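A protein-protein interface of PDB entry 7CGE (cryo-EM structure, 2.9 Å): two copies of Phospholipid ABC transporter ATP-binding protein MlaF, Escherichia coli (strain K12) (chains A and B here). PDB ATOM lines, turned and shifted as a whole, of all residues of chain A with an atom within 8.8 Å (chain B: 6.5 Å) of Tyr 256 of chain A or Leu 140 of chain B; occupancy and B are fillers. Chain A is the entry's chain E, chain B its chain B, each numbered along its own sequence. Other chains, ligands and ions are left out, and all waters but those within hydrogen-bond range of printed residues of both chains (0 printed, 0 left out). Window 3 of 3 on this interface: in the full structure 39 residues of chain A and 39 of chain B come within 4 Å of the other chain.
Gly 133 of chain B touches Phe 254 of chain A (O to O, 3.995 Å).
Gly 133 of chain B touches Arg 255 of chain A.
C of Gly 136 of chain B touches CD2 of Tyr 256 of chain A (3.6 Å).
Ala 137 of chain B touches Tyr 256 of chain A (N to CD2, 3.6 Å).
Tyr 256 of chain A touches Leu 140 of chain B.
Ala 258 of chain A touches Arg 135 of chain B (CB to NH2, 3.7 Å).
Gly 136 of chain B touches Ala 258 of chain A (N to CB, 3.6 Å).
Gly 259 of chain A touches Arg 135 of chain B (O to NH2, 3.9 Å).
The backbone NH (N) of Val 102 of chain B is in hydrogen-bond range of the backbone carbonyl oxygen (O) of Leu 140 of chain B (3.1 Å).
OD1 of Asp 249 of chain A sits at hydrogen-bond distance from N of Phe 254 of chain A (3.1 Å).
Hydrophobic or aromatic side chains of chain A within 4 Å of the printed part of chain B: Phe 254, Tyr 256 and Ala 258.
Hydrophobic or aromatic side chains of chain B within 4 Å of the printed part of chain A: Leu 140.
Among the printed residues, 10 pairs touch across the chains.
No position is printed for both chains.
Of the 10 pairs that touch across the chains among the printed residues, none has its exchanged pair printed and touching as well.
Of chain B, only Gly 133 (3.2 Å), Gly 136 (3.6 Å), Ala 137 (3.6 Å) and Leu 140 (3.6 Å) come within 4 Å of Tyr 256 of chain A.
Of chain A, only Tyr 256 comes within 4 Å of Leu 140 of chain B.
Ala 137 of chain B touches just one residue of chain A: Tyr 256.
Of the printed residues of chain B, Arg 255 of chain A touches Gly 133 (3.8 Å).
Of the printed residues of chain B, Gly 259 of chain A touches Arg 135.
Of the printed residues of chain A, Arg 135 of chain B touches Ala 258 and Gly 259.
Printed residues of chain A within 4 Å of Gly 133 of chain B: Phe 254, Arg 255 and Tyr 256.
Val 252 of chain A touches none of the printed residues of chain B.
The nearest residue of chain A that does not touch Leu 140 of chain B is Pro 257 of chain A (8.3 Å).
The backbone carbonyl oxygen of Gly 133 of chain B is in hydrogen-bond range of the backbone NH of Tyr 256 of chain A (3.2 Å).
The guanidinium group (NH2) of Arg 152 of chain B lies within hydrogen-bond range of the backbone carbonyl oxygen (O) of Phe 254 of chain A, 2.8 Å away.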
ATOM      1  N   ASP A 249     -11.491  17.981 -38.833  1.00  0.00           N
ATOM      2  CA  ASP A 249     -10.135  17.639 -39.233  1.00  0.00           C
ATOM      3  C   ASP A 249      -9.414  18.846 -39.814  1.00  0.00           C
ATOM      4  O   ASP A 249      -9.986  19.636 -40.568  1.00  0.00           O
ATOM      5  CB  ASP A 249     -10.132  16.490 -40.241  1.00  0.00           C
ATOM      6  CG  ASP A 249      -8.822  15.740 -40.258  1.00  0.00           C
ATOM      7  OD1 ASP A 249      -8.343  15.351 -39.172  1.00  0.00           O
ATOM      8  OD2 ASP A 249      -8.275  15.514 -41.359  1.00  0.00           O
ATOM      9  N   VAL A 252      -5.262  20.428 -36.231  1.00  0.00           N
ATOM     10  CA  VAL A 252      -5.460  19.611 -35.036  1.00  0.00           C
ATOM     11  C   VAL A 252      -6.122  18.313 -35.488  1.00  0.00           C
ATOM     12  O   VAL A 252      -7.313  18.332 -35.848  1.00  0.00           O
ATOM     13  CB  VAL A 252      -6.310  20.331 -33.984  1.00  0.00           C
ATOM     14  CG1 VAL A 252      -6.433  19.472 -32.746  1.00  0.00           C
ATOM     15  CG2 VAL A 252      -5.686  21.660 -33.641  1.00  0.00           C
ATOM     16  N   PRO A 253      -5.415  17.188 -35.491  1.00  0.00           N
ATOM     17  CA  PRO A 253      -5.922  15.997 -36.172  1.00  0.00           C
ATOM     18  C   PRO A 253      -7.031  15.299 -35.406  1.00  0.00           C
ATOM     19  O   PRO A 253      -7.068  15.287 -34.175  1.00  0.00           O
ATOM     20  CB  PRO A 253      -4.682  15.110 -36.269  1.00  0.00           C
ATOM     21  CG  PRO A 253      -3.857  15.514 -35.108  1.00  0.00           C
ATOM     22  CD  PRO A 253      -4.078  16.976 -34.921  1.00  0.00           C
ATOM     23  N   PHE A 254      -7.948  14.706 -36.172  1.00  0.00           N
ATOM     24  CA  PHE A 254      -9.043  13.951 -35.577  1.00  0.00           C
ATOM     25  C   PHE A 254      -8.546  12.642 -34.984  1.00  0.00           C
ATOM     26  O   PHE A 254      -9.004  12.225 -33.917  1.00  0.00           O
ATOM     27  CB  PHE A 254     -10.125  13.714 -36.628  1.00  0.00           C
ATOM     28  CG  PHE A 254     -11.014  12.541 -36.350  1.00  0.00           C
ATOM     29  CD1 PHE A 254     -11.926  12.568 -35.314  1.00  0.00           C
ATOM     30  CD2 PHE A 254     -10.962  11.421 -37.154  1.00  0.00           C
ATOM     31  CE1 PHE A 254     -12.746  11.488 -35.072  1.00  0.00           C
ATOM     32  CE2 PHE A 254     -11.784  10.344 -36.914  1.00  0.00           C
ATOM     33  CZ  PHE A 254     -12.673  10.378 -35.874  1.00  0.00           C
ATOM     34  N   ARG A 255      -7.596  11.995 -35.644  1.00  0.00           N
ATOM     35  CA  ARG A 255      -7.027  10.756 -35.147  1.00  0.00           C
ATOM     36  C   ARG A 255      -5.928  11.034 -34.137  1.00  0.00           C
ATOM     37  O   ARG A 255      -5.107  11.933 -34.323  1.00  0.00           O
ATOM     38  CB  ARG A 255      -6.459   9.940 -36.300  1.00  0.00           C
ATOM     39  CG  ARG A 255      -7.489   9.506 -37.300  1.00  0.00           C
ATOM     40  CD  ARG A 255      -8.230   8.312 -36.783  1.00  0.00           C
ATOM     41  NE  ARG A 255      -9.467   8.089 -37.510  1.00  0.00           N
ATOM     42  CZ  ARG A 255      -9.566   7.323 -38.581  1.00  0.00           C
ATOM     43  NH1 ARG A 255      -8.491   6.719 -39.044  1.00  0.00           N
ATOM     44  NH2 ARG A 255     -10.732   7.167 -39.187  1.00  0.00           N
ATOM     45  N   TYR A 256      -5.918  10.255 -33.067  1.00  0.00           N
ATOM     46  CA  TYR A 256      -4.804  10.261 -32.139  1.00  0.00           C
ATOM     47  C   TYR A 256      -3.559   9.719 -32.837  1.00  0.00           C
ATOM     48  O   TYR A 256      -3.667   8.935 -33.781  1.00  0.00           O
ATOM     49  CB  TYR A 256      -5.142   9.405 -30.926  1.00  0.00           C
ATOM     50  CG  TYR A 256      -4.340   9.701 -29.691  1.00  0.00           C
ATOM     51  CD1 TYR A 256      -4.633  10.794 -28.900  1.00  0.00           C
ATOM     52  CD2 TYR A 256      -3.291   8.881 -29.313  1.00  0.00           C
ATOM     53  CE1 TYR A 256      -3.901  11.067 -27.768  1.00  0.00           C
ATOM     54  CE2 TYR A 256      -2.555   9.143 -28.184  1.00  0.00           C
ATOM     55  CZ  TYR A 256      -2.865  10.238 -27.415  1.00  0.00           C
ATOM     56  OH  TYR A 256      -2.135  10.508 -26.285  1.00  0.00           O
ATOM     57  N   PRO A 257      -2.362  10.149 -32.423  1.00  0.00           N
ATOM     58  CA  PRO A 257      -1.148   9.563 -33.003  1.00  0.00           C
ATOM     59  C   PRO A 257      -0.968   8.115 -32.598  1.00  0.00           C
ATOM     60  O   PRO A 257      -0.632   7.804 -31.453  1.00  0.00           O
ATOM     61  CB  PRO A 257      -0.028  10.447 -32.445  1.00  0.00           C
ATOM     62  CG  PRO A 257      -0.633  11.166 -31.300  1.00  0.00           C
ATOM     63  CD  PRO A 257      -2.052  11.373 -31.673  1.00  0.00           C
ATOM     64  N   ALA A 258      -1.186   7.224 -33.550  1.00  0.00           N
ATOM     65  CA  ALA A 258      -1.214   5.793 -33.318  1.00  0.00           C
ATOM     66  C   ALA A 258      -0.023   5.135 -33.993  1.00  0.00           C
ATOM     67  O   ALA A 258       0.806   5.787 -34.630  1.00  0.00           O
ATOM     68  CB  ALA A 258      -2.521   5.195 -33.836  1.00  0.00           C
ATOM     69  N   GLY A 259       0.042   3.817 -33.867  1.00  0.00           N
ATOM     70  CA  GLY A 259       1.027   3.057 -34.597  1.00  0.00           C
ATOM     71  C   GLY A 259       0.493   2.745 -35.973  1.00  0.00           C
ATOM     72  O   GLY A 259       0.104   3.651 -36.714  1.00  0.00           O
ATOM     73  N   MET B 100      -8.452   0.000 -15.103  1.00  0.00           N
ATOM     74  CA  MET B 100      -8.808  -0.582 -16.399  1.00  0.00           C
ATOM     75  C   MET B 100      -8.657   0.374 -17.575  1.00  0.00           C
ATOM     76  O   MET B 100      -9.641   1.013 -17.944  1.00  0.00           O
ATOM     77  CB  MET B 100     -10.241  -1.128 -16.424  1.00  0.00           C
ATOM     78  CG  MET B 100     -10.633  -2.015 -15.287  1.00  0.00           C
ATOM     79  SD  MET B 100     -12.418  -2.204 -15.230  1.00  0.00           S
ATOM     80  CE  MET B 100     -12.779  -2.355 -16.965  1.00  0.00           C
ATOM     81  N   ASN B 101      -7.448   0.546 -18.110  1.00  0.00           N
ATOM     82  CA  ASN B 101      -7.160   1.405 -19.262  1.00  0.00           C
ATOM     83  C   ASN B 101      -8.092   1.223 -20.459  1.00  0.00           C
ATOM     84  O   ASN B 101      -8.783   0.208 -20.550  1.00  0.00           O
ATOM     85  CB  ASN B 101      -5.743   1.132 -19.741  1.00  0.00           C
ATOM     86  CG  ASN B 101      -5.593  -0.249 -20.312  1.00  0.00           C
ATOM     87  OD1 ASN B 101      -6.041  -1.219 -19.721  1.00  0.00           O
ATOM     88  ND2 ASN B 101      -4.976  -0.348 -21.473  1.00  0.00           N
ATOM     89  N   VAL B 102      -8.078   2.194 -21.383  1.00  0.00           N
ATOM     90  CA  VAL B 102      -9.077   2.401 -22.442  1.00  0.00           C
ATOM     91  C   VAL B 102      -9.406   1.141 -23.240  1.00  0.00           C
ATOM     92  O   VAL B 102     -10.557   0.942 -23.644  1.00  0.00           O
ATOM     93  CB  VAL B 102      -8.583   3.551 -23.350  1.00  0.00           C
ATOM     94  CG1 VAL B 102      -9.492   3.805 -24.528  1.00  0.00           C
ATOM     95  CG2 VAL B 102      -8.481   4.810 -22.549  1.00  0.00           C
ATOM     96  N   PHE B 103      -8.438   0.240 -23.416  1.00  0.00           N
ATOM     97  CA  PHE B 103      -8.731  -1.057 -24.020  1.00  0.00           C
ATOM     98  C   PHE B 103      -9.653  -1.886 -23.138  1.00  0.00           C
ATOM     99  O   PHE B 103     -10.586  -2.520 -23.635  1.00  0.00           O
ATOM    100  CB  PHE B 103      -7.435  -1.818 -24.286  1.00  0.00           C
ATOM    101  CG  PHE B 103      -7.620  -3.090 -25.067  1.00  0.00           C
ATOM    102  CD1 PHE B 103      -7.612  -3.071 -26.443  1.00  0.00           C
ATOM    103  CD2 PHE B 103      -7.781  -4.307 -24.425  1.00  0.00           C
ATOM    104  CE1 PHE B 103      -7.776  -4.232 -27.163  1.00  0.00           C
ATOM    105  CE2 PHE B 103      -7.956  -5.462 -25.141  1.00  0.00           C
ATOM    106  CZ  PHE B 103      -7.949  -5.425 -26.509  1.00  0.00           C
ATOM    107  N   GLY B 133     -11.529   7.087 -33.440  1.00  0.00           N
ATOM    108  CA  GLY B 133     -10.261   7.766 -33.591  1.00  0.00           C
ATOM    109  C   GLY B 133      -9.342   7.730 -32.397  1.00  0.00           C
ATOM    110  O   GLY B 133      -8.526   8.632 -32.236  1.00  0.00           O
ATOM    111  N   LEU B 134      -9.431   6.705 -31.561  1.00  0.00           N
ATOM    112  CA  LEU B 134      -8.613   6.615 -30.359  1.00  0.00           C
ATOM    113  C   LEU B 134      -7.865   5.303 -30.298  1.00  0.00           C
ATOM    114  O   LEU B 134      -7.692   4.727 -29.226  1.00  0.00           O
ATOM    115  CB  LEU B 134      -9.450   6.776 -29.095  1.00  0.00           C
ATOM    116  CG  LEU B 134      -9.702   8.150 -28.490  1.00  0.00           C
ATOM    117  CD1 LEU B 134     -10.635   8.951 -29.319  1.00  0.00           C
ATOM    118  CD2 LEU B 134     -10.283   7.958 -27.129  1.00  0.00           C
ATOM    119  N   ARG B 135      -7.403   4.804 -31.441  1.00  0.00           N
ATOM    120  CA  ARG B 135      -6.660   3.550 -31.436  1.00  0.00           C
ATOM    121  C   ARG B 135      -5.277   3.720 -30.824  1.00  0.00           C
ATOM    122  O   ARG B 135      -4.742   2.776 -30.237  1.00  0.00           O
ATOM    123  CB  ARG B 135      -6.549   3.002 -32.851  1.00  0.00           C
ATOM    124  CG  ARG B 135      -6.149   1.560 -32.899  1.00  0.00           C
ATOM    125  CD  ARG B 135      -6.173   1.015 -34.303  1.00  0.00           C
ATOM    126  NE  ARG B 135      -5.479   1.881 -35.243  1.00  0.00           N
ATOM    127  CZ  ARG B 135      -4.171   1.861 -35.446  1.00  0.00           C
ATOM    128  NH1 ARG B 135      -3.405   1.021 -34.771  1.00  0.00           N
ATOM    129  NH2 ARG B 135      -3.628   2.682 -36.326  1.00  0.00           N
ATOM    130  N   GLY B 136      -4.689   4.908 -30.934  1.00  0.00           N
ATOM    131  CA  GLY B 136      -3.420   5.150 -30.282  1.00  0.00           C
ATOM    132  C   GLY B 136      -3.517   5.336 -28.790  1.00  0.00           C
ATOM    133  O   GLY B 136      -2.521   5.153 -28.088  1.00  0.00           O
ATOM    134  N   ALA B 137      -4.696   5.684 -28.288  1.00  0.00           N
ATOM    135  CA  ALA B 137      -4.904   5.914 -26.870  1.00  0.00           C
ATOM    136  C   ALA B 137      -5.346   4.665 -26.138  1.00  0.00           C
ATOM    137  O   ALA B 137      -5.988   4.772 -25.093  1.00  0.00           O
ATOM    138  CB  ALA B 137      -5.931   7.023 -26.663  1.00  0.00           C
ATOM    139  N   ALA B 138      -5.008   3.487 -26.656  1.00  0.00           N
ATOM    140  CA  ALA B 138      -5.568   2.252 -26.134  1.00  0.00           C
ATOM    141  C   ALA B 138      -4.970   1.852 -24.798  1.00  0.00           C
ATOM    142  O   ALA B 138      -5.589   1.075 -24.070  1.00  0.00           O
ATOM    143  CB  ALA B 138      -5.375   1.130 -27.145  1.00  0.00           C
ATOM    144  N   LYS B 139      -3.793   2.357 -24.453  1.00  0.00           N
ATOM    145  CA  LYS B 139      -3.138   1.984 -23.211  1.00  0.00           C
ATOM    146  C   LYS B 139      -3.122   3.098 -22.183  1.00  0.00           C
ATOM    147  O   LYS B 139      -2.553   2.916 -21.106  1.00  0.00           O
ATOM    148  CB  LYS B 139      -1.709   1.523 -23.491  1.00  0.00           C
ATOM    149  CG  LYS B 139      -1.632   0.201 -24.216  1.00  0.00           C
ATOM    150  CD  LYS B 139      -0.208  -0.304 -24.284  1.00  0.00           C
ATOM    151  CE  LYS B 139       0.692   0.693 -24.988  1.00  0.00           C
ATOM    152  NZ  LYS B 139       2.116   0.261 -24.994  1.00  0.00           N
ATOM    153  N   LEU B 140      -3.725   4.240 -22.479  1.00  0.00           N
ATOM    154  CA  LEU B 140      -3.809   5.313 -21.507  1.00  0.00           C
ATOM    155  C   LEU B 140      -4.852   4.988 -20.453  1.00  0.00           C
ATOM    156  O   LEU B 140      -5.807   4.259 -20.703  1.00  0.00           O
ATOM    157  CB  LEU B 140      -4.166   6.626 -22.190  1.00  0.00           C
ATOM    158  CG  LEU B 140      -3.175   7.159 -23.213  1.00  0.00           C
ATOM    159  CD1 LEU B 140      -3.683   8.458 -23.769  1.00  0.00           C
ATOM    160  CD2 LEU B 140      -1.829   7.354 -22.576  1.00  0.00           C
ATOM    161  N   MET B 141      -4.659   5.519 -19.289  1.00  0.00           N
ATOM    162  CA  MET B 141      -5.655   5.418 -18.242  1.00  0.00           C
ATOM    163  C   MET B 141      -6.678   6.531 -18.409  1.00  0.00           C
ATOM    164  O   MET B 141      -6.389   7.548 -19.039  1.00  0.00           O
ATOM    165  CB  MET B 141      -4.979   5.497 -16.878  1.00  0.00           C
ATOM    166  CG  MET B 141      -3.992   4.381 -16.639  1.00  0.00           C
ATOM    167  SD  MET B 141      -4.736   2.746 -16.613  1.00  0.00           S
ATOM    168  CE  MET B 141      -5.513   2.743 -15.007  1.00  0.00           C
ATOM    169  N   PRO B 142      -7.900   6.366 -17.888  1.00  0.00           N
ATOM    170  CA  PRO B 142      -8.908   7.423 -18.039  1.00  0.00           C
ATOM    171  C   PRO B 142      -8.607   8.704 -17.287  1.00  0.00           C
ATOM    172  O   PRO B 142      -9.257   9.715 -17.565  1.00  0.00           O
ATOM    173  CB  PRO B 142     -10.180   6.766 -17.497  1.00  0.00           C
ATOM    174  CG  PRO B 142      -9.700   5.694 -16.652  1.00  0.00           C
ATOM    175  CD  PRO B 142      -8.521   5.148 -17.354  1.00  0.00           C
ATOM    176  N   SER B 143      -7.660   8.711 -16.355  1.00  0.00           N
ATOM    177  CA  SER B 143      -7.312   9.953 -15.685  1.00  0.00           C
ATOM    178  C   SER B 143      -6.430  10.848 -16.537  1.00  0.00           C
ATOM    179  O   SER B 143      -6.208  12.002 -16.167  1.00  0.00           O
ATOM    180  CB  SER B 143      -6.607   9.674 -14.363  1.00  0.00           C
ATOM    181  OG  SER B 143      -5.314   9.144 -14.582  1.00  0.00           O
ATOM    182  N   GLU B 144      -5.934  10.357 -17.666  1.00  0.00           N
ATOM    183  CA  GLU B 144      -5.079  11.131 -18.552  1.00  0.00           C
ATOM    184  C   GLU B 144      -5.792  11.492 -19.848  1.00  0.00           C
ATOM    185  O   GLU B 144      -5.145  11.785 -20.851  1.00  0.00           O
ATOM    186  CB  GLU B 144      -3.808  10.352 -18.863  1.00  0.00           C
ATOM    187  CG  GLU B 144      -3.277   9.552 -17.701  1.00  0.00           C
ATOM    188  CD  GLU B 144      -2.376   8.420 -18.145  1.00  0.00           C
ATOM    189  OE1 GLU B 144      -2.190   8.257 -19.362  1.00  0.00           O
ATOM    190  OE2 GLU B 144      -1.868   7.679 -17.280  1.00  0.00           O
ATOM    191  N   LEU B 145      -7.123  11.473 -19.849  1.00  0.00           N
ATOM    192  CA  LEU B 145      -7.848  11.387 -21.105  1.00  0.00           C
ATOM    193  C   LEU B 145      -8.414  12.688 -21.639  1.00  0.00           C
ATOM    194  O   LEU B 145      -8.907  12.664 -22.768  1.00  0.00           O
ATOM    195  CB  LEU B 145      -8.991  10.382 -21.022  1.00  0.00           C
ATOM    196  CG  LEU B 145      -8.682   9.038 -21.662  1.00  0.00           C
ATOM    197  CD1 LEU B 145      -9.898   8.166 -21.610  1.00  0.00           C
ATOM    198  CD2 LEU B 145      -8.238   9.236 -23.089  1.00  0.00           C
ATOM    199  N   MET B 149     -12.150  13.736 -24.963  1.00  0.00           N
ATOM    200  CA  MET B 149     -11.840  12.411 -25.476  1.00  0.00           C
ATOM    201  C   MET B 149     -12.353  11.295 -24.592  1.00  0.00           C
ATOM    202  O   MET B 149     -12.317  10.138 -25.007  1.00  0.00           O
ATOM    203  CB  MET B 149     -10.336  12.240 -25.638  1.00  0.00           C
ATOM    204  CG  MET B 149      -9.751  12.948 -26.816  1.00  0.00           C
ATOM    205  SD  MET B 149      -8.149  12.262 -27.245  1.00  0.00           S
ATOM    206  CE  MET B 149      -7.306  12.372 -25.673  1.00  0.00           C
ATOM    207  N   ARG B 152     -15.484  10.210 -26.272  1.00  0.00           N
ATOM    208  CA  ARG B 152     -15.265   9.387 -27.450  1.00  0.00           C
ATOM    209  C   ARG B 152     -14.891   7.966 -27.083  1.00  0.00           C
ATOM    210  O   ARG B 152     -15.247   7.037 -27.805  1.00  0.00           O
ATOM    211  CB  ARG B 152     -14.170   9.983 -28.321  1.00  0.00           C
ATOM    212  CG  ARG B 152     -14.567  11.215 -29.049  1.00  0.00           C
ATOM    213  CD  ARG B 152     -13.358  12.039 -29.348  1.00  0.00           C
ATOM    214  NE  ARG B 152     -12.629  11.544 -30.500  1.00  0.00           N
ATOM    215  CZ  ARG B 152     -11.463  12.030 -30.893  1.00  0.00           C
ATOM    216  NH1 ARG B 152     -10.901  13.012 -30.217  1.00  0.00           N
ATOM    217  NH2 ARG B 152     -10.861  11.534 -31.955  1.00  0.00           N
